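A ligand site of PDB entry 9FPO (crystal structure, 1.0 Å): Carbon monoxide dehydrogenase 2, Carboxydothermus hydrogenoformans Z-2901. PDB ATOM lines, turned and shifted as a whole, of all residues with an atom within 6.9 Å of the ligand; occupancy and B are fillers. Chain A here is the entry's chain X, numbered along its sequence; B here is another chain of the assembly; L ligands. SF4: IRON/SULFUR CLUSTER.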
ATOM      1  N   CYS A  47     -10.276 -25.950  17.807  1.00  0.00           N
ATOM      2  CA  CYS A  47      -9.669 -25.276  16.672  1.00  0.00           C
ATOM      3  C   CYS A  47      -8.231 -25.791  16.561  1.00  0.00           C
ATOM      4  O   CYS A  47      -7.538 -25.946  17.579  1.00  0.00           O
ATOM      5  CB  CYS A  47      -9.676 -23.769  16.829  1.00  0.00           C
ATOM      6  SG  CYS A  47      -8.860 -22.942  15.407  1.00  0.00           S
ATOM      7  N   CYS A  48      -7.781 -26.019  15.318  1.00  0.00           N
ATOM      8  CA  CYS A  48      -6.412 -26.439  15.040  1.00  0.00           C
ATOM      9  C   CYS A  48      -5.876 -25.660  13.858  1.00  0.00           C
ATOM     10  O   CYS A  48      -6.542 -25.584  12.808  1.00  0.00           O
ATOM     11  CB  CYS A  48      -6.366 -27.928  14.743  1.00  0.00           C
ATOM     12  SG  CYS A  48      -4.688 -28.543  14.429  1.00  0.00           S
ATOM     13  N   ARG A  49      -4.674 -25.132  14.029  1.00  0.00           N
ATOM     14  CA  ARG A  49      -3.925 -24.440  12.990  1.00  0.00           C
ATOM     15  C   ARG A  49      -2.523 -25.065  12.840  1.00  0.00           C
ATOM     16  O   ARG A  49      -1.567 -24.358  12.515  1.00  0.00           O
ATOM     17  CB  ARG A  49      -3.858 -22.945  13.282  1.00  0.00           C
ATOM     18  CG  ARG A  49      -5.193 -22.273  13.270  1.00  0.00           C
ATOM     19  CD  ARG A  49      -5.089 -20.904  13.868  1.00  0.00           C
ATOM     20  NE  ARG A  49      -4.235 -20.066  13.067  1.00  0.00           N
ATOM     21  CZ  ARG A  49      -3.608 -18.989  13.476  1.00  0.00           C
ATOM     22  NH1 ARG A  49      -3.828 -18.483  14.670  1.00  0.00           N
ATOM     23  NH2 ARG A  49      -2.825 -18.316  12.622  1.00  0.00           N
ATOM     24  N   HIS A  50      -2.415 -26.357  13.078  1.00  0.00           N
ATOM     25  CA  HIS A  50      -1.119 -27.015  13.054  1.00  0.00           C
ATOM     26  C   HIS A  50      -0.620 -27.351  11.647  1.00  0.00           C
ATOM     27  O   HIS A  50       0.508 -27.835  11.537  1.00  0.00           O
ATOM     28  CB  HIS A  50      -1.056 -28.237  13.960  1.00  0.00           C
ATOM     29  CG  HIS A  50      -1.197 -27.893  15.428  1.00  0.00           C
ATOM     30  ND1 HIS A  50      -0.858 -28.774  16.415  1.00  0.00           N
ATOM     31  CD2 HIS A  50      -1.638 -26.783  16.080  1.00  0.00           C
ATOM     32  CE1 HIS A  50      -1.097 -28.229  17.605  1.00  0.00           C
ATOM     33  NE2 HIS A  50      -1.572 -27.009  17.439  1.00  0.00           N
ATOM     34  N   CYS A  51      -1.371 -27.068  10.599  1.00  0.00           N
ATOM     35  CA  CYS A  51      -0.814 -27.166   9.260  1.00  0.00           C
ATOM     36  C   CYS A  51      -1.568 -26.196   8.356  1.00  0.00           C
ATOM     37  O   CYS A  51      -2.578 -25.605   8.729  1.00  0.00           O
ATOM     38  CB  CYS A  51      -0.816 -28.593   8.696  1.00  0.00           C
ATOM     39  SG  CYS A  51      -2.425 -29.163   8.028  1.00  0.00           S
ATOM     40  N   LEU A  52      -1.059 -26.077   7.121  1.00  0.00           N
ATOM     41  CA  LEU A  52      -1.591 -25.128   6.157  1.00  0.00           C
ATOM     42  C   LEU A  52      -2.826 -25.636   5.414  1.00  0.00           C
ATOM     43  O   LEU A  52      -3.333 -24.918   4.541  1.00  0.00           O
ATOM     44  CB  LEU A  52      -0.478 -24.693   5.189  1.00  0.00           C
ATOM     45  CG  LEU A  52       0.747 -24.080   5.794  1.00  0.00           C
ATOM     46  CD1 LEU A  52       1.721 -23.726   4.694  1.00  0.00           C
ATOM     47  CD2 LEU A  52       0.351 -22.875   6.647  1.00  0.00           C
ATOM     48  N   GLN A  53      -3.340 -26.814   5.756  1.00  0.00           N
ATOM     49  CA  GLN A  53      -4.684 -27.174   5.344  1.00  0.00           C
ATOM     50  C   GLN A  53      -5.745 -26.546   6.228  1.00  0.00           C
ATOM     51  O   GLN A  53      -6.902 -26.449   5.809  1.00  0.00           O
ATOM     52  CB  GLN A  53      -4.910 -28.687   5.325  1.00  0.00           C
ATOM     53  CG  GLN A  53      -4.060 -29.351   4.270  1.00  0.00           C
ATOM     54  CD  GLN A  53      -4.143 -30.843   4.137  1.00  0.00           C
ATOM     55  OE1 GLN A  53      -3.883 -31.374   3.069  1.00  0.00           O
ATOM     56  NE2 GLN A  53      -4.558 -31.551   5.181  1.00  0.00           N
ATOM     57  N   GLY A  54      -5.358 -26.075   7.414  1.00  0.00           N
ATOM     58  CA  GLY A  54      -6.270 -25.401   8.291  1.00  0.00           C
ATOM     59  C   GLY A  54      -6.531 -23.980   7.872  1.00  0.00           C
ATOM     60  O   GLY A  54      -6.078 -23.525   6.822  1.00  0.00           O
ATOM     61  N   PRO A  55      -7.245 -23.244   8.712  1.00  0.00           N
ATOM     62  CA  PRO A  55      -7.681 -23.621  10.073  1.00  0.00           C
ATOM     63  C   PRO A  55      -8.796 -24.665  10.020  1.00  0.00           C
ATOM     64  O   PRO A  55      -9.735 -24.582   9.213  1.00  0.00           O
ATOM     65  CB  PRO A  55      -8.146 -22.289  10.653  1.00  0.00           C
ATOM     66  CG  PRO A  55      -8.635 -21.515   9.436  1.00  0.00           C
ATOM     67  CD  PRO A  55      -7.654 -21.860   8.375  1.00  0.00           C
ATOM     68  N   CYS A  56      -8.733 -25.595  10.954  1.00  0.00           N
ATOM     69  CA  CYS A  56      -9.781 -26.567  11.185  1.00  0.00           C
ATOM     70  C   CYS A  56     -10.481 -26.243  12.484  1.00  0.00           C
ATOM     71  O   CYS A  56      -9.895 -25.693  13.441  1.00  0.00           O
ATOM     72  CB  CYS A  56      -9.186 -27.961  11.274  1.00  0.00           C
ATOM     73  SG  CYS A  56      -8.588 -28.572   9.680  1.00  0.00           S
ATOM     74  N   ARG A  57     -11.757 -26.604  12.548  1.00  0.00           N
ATOM     75  CA  ARG A  57     -12.562 -26.461  13.746  1.00  0.00           C
ATOM     76  C   ARG A  57     -13.517 -27.644  13.803  1.00  0.00           C
ATOM     77  O   ARG A  57     -13.763 -28.310  12.799  1.00  0.00           O
ATOM     78  CB  ARG A  57     -13.325 -25.135  13.764  1.00  0.00           C
ATOM     79  CG  ARG A  57     -14.535 -25.084  12.844  1.00  0.00           C
ATOM     80  CD  ARG A  57     -14.860 -23.679  12.366  1.00  0.00           C
ATOM     81  NE  ARG A  57     -15.992 -23.673  11.462  1.00  0.00           N
ATOM     82  CZ  ARG A  57     -15.955 -24.075  10.192  1.00  0.00           C
ATOM     83  NH1 ARG A  57     -14.796 -24.222   9.578  1.00  0.00           N
ATOM     84  NH2 ARG A  57     -17.070 -24.380   9.566  1.00  0.00           N
ATOM     85  N   VAL A  67     -14.701 -33.366  12.536  1.00  0.00           N
ATOM     86  CA  VAL A  67     -13.354 -33.915  12.569  1.00  0.00           C
ATOM     87  C   VAL A  67     -12.476 -32.977  11.763  1.00  0.00           C
ATOM     88  O   VAL A  67     -12.934 -32.331  10.836  1.00  0.00           O
ATOM     89  CB  VAL A  67     -13.420 -35.359  12.017  1.00  0.00           C
ATOM     90  CG1 VAL A  67     -13.939 -35.420  10.601  1.00  0.00           C
ATOM     91  CG2 VAL A  67     -12.145 -36.075  12.206  1.00  0.00           C
ATOM     92  N   GLY A  68     -11.195 -32.920  12.126  1.00  0.00           N
ATOM     93  CA  GLY A  68     -10.276 -32.129  11.348  1.00  0.00           C
ATOM     94  C   GLY A  68     -10.029 -32.721   9.978  1.00  0.00           C
ATOM     95  O   GLY A  68     -10.296 -33.881   9.699  1.00  0.00           O
ATOM     96  N   ILE A  69      -9.442 -31.907   9.093  1.00  0.00           N
ATOM     97  CA  ILE A  69      -9.244 -32.309   7.697  1.00  0.00           C
ATOM     98  C   ILE A  69      -8.387 -33.556   7.602  1.00  0.00           C
ATOM     99  O   ILE A  69      -8.672 -34.448   6.793  1.00  0.00           O
ATOM    100  CB  ILE A  69      -8.729 -31.142   6.856  1.00  0.00           C
ATOM    101  CG1 ILE A  69      -9.839 -30.114   6.685  1.00  0.00           C
ATOM    102  CG2 ILE A  69      -8.205 -31.657   5.527  1.00  0.00           C
ATOM    103  CD1 ILE A  69      -9.407 -28.810   6.075  1.00  0.00           C
ATOM    104  N   CYS A  70      -7.324 -33.660   8.410  1.00  0.00           N
ATOM    105  CA  CYS A  70      -6.447 -34.830   8.403  1.00  0.00           C
ATOM    106  C   CYS A  70      -7.060 -36.043   9.122  1.00  0.00           C
ATOM    107  O   CYS A  70      -6.441 -37.109   9.135  1.00  0.00           O
ATOM    108  CB  CYS A  70      -5.097 -34.485   9.024  1.00  0.00           C
ATOM    109  SG  CYS A  70      -5.313 -33.998  10.777  1.00  0.00           S
ATOM    110  N   GLY A  71      -8.224 -35.856   9.726  1.00  0.00           N
ATOM    111  CA  GLY A  71      -8.847 -36.878  10.543  1.00  0.00           C
ATOM    112  C   GLY A  71      -8.683 -36.674  12.045  1.00  0.00           C
ATOM    113  O   GLY A  71      -9.152 -37.501  12.825  1.00  0.00           O
ATOM    114  N   ALA A  72      -8.026 -35.597  12.467  1.00  0.00           N
ATOM    115  CA  ALA A  72      -7.825 -35.384  13.896  1.00  0.00           C
ATOM    116  C   ALA A  72      -9.171 -35.191  14.596  1.00  0.00           C
ATOM    117  O   ALA A  72      -9.978 -34.339  14.219  1.00  0.00           O
ATOM    118  CB  ALA A  72      -6.947 -34.152  14.131  1.00  0.00           C
ATOM    119  N   THR A  73      -9.379 -35.963  15.649  1.00  0.00           N
ATOM    120  CA  THR A  73     -10.617 -35.919  16.406  1.00  0.00           C
ATOM    121  C   THR A  73     -10.586 -34.729  17.390  1.00  0.00           C
ATOM    122  O   THR A  73      -9.541 -34.108  17.634  1.00  0.00           O
ATOM    123  CB  THR A  73     -10.834 -37.179  17.216  1.00  0.00           C
ATOM    124  OG1 THR A  73      -9.734 -37.274  18.126  1.00  0.00           O
ATOM    125  CG2 THR A  73     -10.946 -38.423  16.325  1.00  0.00           C
ATOM    126  N   ILE A  77      -7.271 -32.880  18.927  1.00  0.00           N
ATOM    127  CA  ILE A  77      -7.050 -31.448  18.769  1.00  0.00           C
ATOM    128  C   ILE A  77      -6.952 -30.762  20.125  1.00  0.00           C
ATOM    129  O   ILE A  77      -6.040 -29.965  20.382  1.00  0.00           O
ATOM    130  CB  ILE A  77      -8.165 -30.864  17.903  1.00  0.00           C
ATOM    131  CG1 ILE A  77      -7.970 -31.283  16.429  1.00  0.00           C
ATOM    132  CG2 ILE A  77      -8.318 -29.342  18.083  1.00  0.00           C
ATOM    133  CD1 ILE A  77      -9.168 -30.873  15.535  1.00  0.00           C
ATOM    134  N   ARG A  80      -3.616 -31.801  21.840  1.00  0.00           N
ATOM    135  CA  ARG A  80      -2.450 -31.191  21.205  1.00  0.00           C
ATOM    136  C   ARG A  80      -2.307 -29.718  21.581  1.00  0.00           C
ATOM    137  O   ARG A  80      -1.205 -29.248  21.835  1.00  0.00           O
ATOM    138  CB  ARG A  80      -2.483 -31.345  19.690  1.00  0.00           C
ATOM    139  CG  ARG A  80      -2.368 -32.813  19.234  1.00  0.00           C
ATOM    140  CD  ARG A  80      -2.124 -32.978  17.735  1.00  0.00           C
ATOM    141  NE  ARG A  80      -3.108 -32.302  16.932  1.00  0.00           N
ATOM    142  CZ  ARG A  80      -3.246 -32.533  15.631  1.00  0.00           C
ATOM    143  NH1 ARG A  80      -2.502 -33.405  15.006  1.00  0.00           N
ATOM    144  NH2 ARG A  80      -4.163 -31.880  14.943  1.00  0.00           N
ATOM    145  N   THR A 197       2.942 -33.082  18.597  1.00  0.00           N
ATOM    146  CA  THR A 197       1.716 -32.363  18.361  1.00  0.00           C
ATOM    147  C   THR A 197       1.633 -31.771  16.958  1.00  0.00           C
ATOM    148  O   THR A 197       0.576 -31.224  16.598  1.00  0.00           O
ATOM    149  CB  THR A 197       1.513 -31.261  19.400  1.00  0.00           C
ATOM    150  OG1 THR A 197       2.607 -30.359  19.337  1.00  0.00           O
ATOM    151  CG2 THR A 197       1.344 -31.811  20.810  1.00  0.00           C
ATOM    152  N   SER A 198       2.698 -31.871  16.168  1.00  0.00           N
ATOM    153  CA  SER A 198       2.683 -31.449  14.785  1.00  0.00           C
ATOM    154  C   SER A 198       1.834 -32.427  13.963  1.00  0.00           C
ATOM    155  O   SER A 198       1.457 -33.516  14.418  1.00  0.00           O
ATOM    156  CB  SER A 198       4.081 -31.284  14.234  1.00  0.00           C
ATOM    157  OG  SER A 198       4.758 -32.479  13.962  1.00  0.00           O
ATOM    158  N   MET A 199       1.495 -32.004  12.738  1.00  0.00           N
ATOM    159  CA  MET A 199       0.522 -32.773  11.971  1.00  0.00           C
ATOM    160  C   MET A 199       1.024 -34.197  11.698  1.00  0.00           C
ATOM    161  O   MET A 199       2.203 -34.435  11.373  1.00  0.00           O
ATOM    162  CB  MET A 199       0.182 -32.015  10.685  1.00  0.00           C
ATOM    163  CG  MET A 199      -0.851 -32.710   9.769  1.00  0.00           C
ATOM    164  SD  MET A 199      -0.060 -34.025   8.768  1.00  0.00           S
ATOM    165  CE  MET A 199      -1.358 -35.218   8.581  1.00  0.00           C
ATOM    166  N   GLY A 200       0.115 -35.139  11.865  1.00  0.00           N
ATOM    167  CA  GLY A 200       0.394 -36.501  11.458  1.00  0.00           C
ATOM    168  C   GLY A 200       1.303 -37.249  12.384  1.00  0.00           C
ATOM    169  O   GLY A 200       1.963 -38.204  11.933  1.00  0.00           O
ATOM    170  N   VAL B  28      -9.999 -37.385   3.014  1.00  0.00           N
ATOM    171  CA  VAL B  28      -9.495 -36.034   3.304  1.00  0.00           C
ATOM    172  C   VAL B  28     -10.239 -34.971   2.503  1.00  0.00           C
ATOM    173  O   VAL B  28     -10.481 -33.867   3.007  1.00  0.00           O
ATOM    174  CB  VAL B  28      -7.968 -35.998   3.077  1.00  0.00           C
ATOM    175  CG1 VAL B  28      -7.578 -36.259   1.604  1.00  0.00           C
ATOM    176  CG2 VAL B  28      -7.333 -34.698   3.558  1.00  0.00           C
ATOM    177  N   MET B  35     -15.413 -28.730   6.067  1.00  0.00           N
ATOM    178  CA  MET B  35     -14.803 -27.634   6.829  1.00  0.00           C
ATOM    179  C   MET B  35     -15.100 -26.255   6.235  1.00  0.00           C
ATOM    180  O   MET B  35     -14.824 -25.235   6.859  1.00  0.00           O
ATOM    181  CB  MET B  35     -13.298 -27.877   6.897  1.00  0.00           C
ATOM    182  CG  MET B  35     -12.599 -27.118   8.030  1.00  0.00           C
ATOM    183  SD  MET B  35     -13.203 -27.594   9.672  1.00  0.00           S
ATOM    184  CE  MET B  35     -12.585 -29.255   9.789  1.00  0.00           C
ATOM    185  N   GLN B  38     -13.759 -22.041   5.730  1.00  0.00           N
ATOM    186  CA  GLN B  38     -12.806 -22.001   6.830  1.00  0.00           C
ATOM    187  C   GLN B  38     -12.741 -20.619   7.462  1.00  0.00           C
ATOM    188  O   GLN B  38     -13.087 -19.605   6.845  1.00  0.00           O
ATOM    189  CB  GLN B  38     -11.446 -22.475   6.347  1.00  0.00           C
ATOM    190  CG  GLN B  38     -11.443 -23.959   5.986  1.00  0.00           C
ATOM    191  CD  GLN B  38     -10.151 -24.472   5.468  1.00  0.00           C
ATOM    192  OE1 GLN B  38      -9.822 -24.279   4.287  1.00  0.00           O
ATOM    193  NE2 GLN B  38      -9.371 -25.082   6.323  1.00  0.00           N
ATOM    194  N   PRO B 336      -4.423 -39.203  10.664  1.00  0.00           N
ATOM    195  CA  PRO B 336      -4.918 -40.167  11.658  1.00  0.00           C
ATOM    196  C   PRO B 336      -6.191 -40.865  11.218  1.00  0.00           C
ATOM    197  O   PRO B 336      -6.536 -41.900  11.804  1.00  0.00           O
ATOM    198  CB  PRO B 336      -5.029 -39.358  12.934  1.00  0.00           C
ATOM    199  CG  PRO B 336      -5.215 -37.966  12.455  1.00  0.00           C
ATOM    200  CD  PRO B 336      -4.313 -37.854  11.256  1.00  0.00           C
ATOM    201  N   MET B 560       2.136 -27.912   3.095  1.00  0.00           N
ATOM    202  CA  MET B 560       1.165 -28.267   4.150  1.00  0.00           C
ATOM    203  C   MET B 560       1.769 -28.234   5.546  1.00  0.00           C
ATOM    204  O   MET B 560       1.271 -27.528   6.438  1.00  0.00           O
ATOM    205  CB  MET B 560       0.525 -29.643   3.846  1.00  0.00           C
ATOM    206  CG  MET B 560      -0.475 -30.195   4.851  1.00  0.00           C
ATOM    207  SD  MET B 560       0.228 -31.155   6.207  1.00  0.00           S
ATOM    208  CE  MET B 560       0.943 -32.531   5.310  1.00  0.00           C
HETATM  209 FE1  SF4 L   1      -6.509 -29.398  10.238  1.00  0.00          FE
HETATM  210 FE2  SF4 L   1      -3.845 -29.498   9.791  1.00  0.00          FE
HETATM  211 FE3  SF4 L   1      -4.840 -29.407  12.292  1.00  0.00          FE
HETATM  212 FE4  SF4 L   1      -5.173 -31.701  10.885  1.00  0.00          FE
HETATM  213  S1  SF4 L   1      -3.190 -30.761  11.633  1.00  0.00           S
HETATM  214  S2  SF4 L   1      -6.745 -30.688  12.155  1.00  0.00           S
HETATM  215  S3  SF4 L   1      -5.501 -30.768   8.772  1.00  0.00           S
HETATM  216  S4  SF4 L   1      -4.952 -27.758  10.707  1.00  0.00           S
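The backbone NH (N) of Gln 53 sits close to the side-chain sulfur (SG) of Cys 51, 3.4 Å away.
The side-chain sulfur (SD) of Met 560 of chain B lies close to the side-chain sulfur (SG) of Cys 51 (3.8 Å).
The backbone NH (N) of Ala 72 sits close to the side-chain sulfur (SG) of Cys 70, at 3.6 Å.
The backbone NH of Cys 48 sits at hydrogen-bond distance from the backbone carbonyl oxygen of Cys 56 (2.8 Å).
The backbone NH (N) of Ile 69 lies close to the side-chain sulfur (SG) of Cys 56 (3.5 Å).
SG of Cys 47 sits close to O of Cys 56.
The backbone carbonyl oxygen (O) of Thr 197 is in hydrogen-bond range of a ring nitrogen (ND1) of His 50, 2.8 Å away.
The backbone carbonyl oxygen of Gln 53 sits at hydrogen-bond distance from the side-chain amide nitrogen of Gln 38 of chain B, 2.9 Å away.
A sulfur (S4) of the ligand sits close to the backbone NH (N) of Cys 51 (3.6 Å).
An iron atom (FE2) of the ligand is bound by the side-chain sulfur (SG) of Cys 51 (2.3 Å).
A sulfur (S3) of the ligand sits close to the backbone NH of Cys 70, 3.4 Å away.
FE4 of the ligand is bound by SG of Cys 70 (2.3 Å).
SG of Cys 56 binds FE1 of the ligand (2.3 Å).
The side-chain sulfur (SG) of Cys 48 binds an iron atom (FE3) of the ligand (2.3 Å).
A sulfur (S4) of the ligand sits close to the backbone NH (N) of Gly 54, 3.7 Å away.
The guanidinium group (NH2) of Arg 80 sits close to a sulfur (S1) of the ligand.
N of His 50 sits close to S4 of the ligand.
The side-chain amide nitrogen of Gln 53 sits close to a sulfur (S3) of the ligand (3.8 Å).
CA of Gly 68 touches S2 of the ligand, at 3.9 Å.
Ile 69 touches the ligand (CB to S3, 3.8 Å).
CB of Ala 72 touches S2 of the ligand, 3.99 Å away.
CG of Met 199 touches S1 of the ligand, 3.6 Å away.
Within 4 Å of the ligand: Cys 48, His 50, Cys 51, Gln 53, Gly 54, Cys 56, Gly 68, Ile 69, Cys 70, Ala 72, Arg 80 and Met 199.
The nearest printed residue that does not touch the ligand is Arg 49 (4.2 Å).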
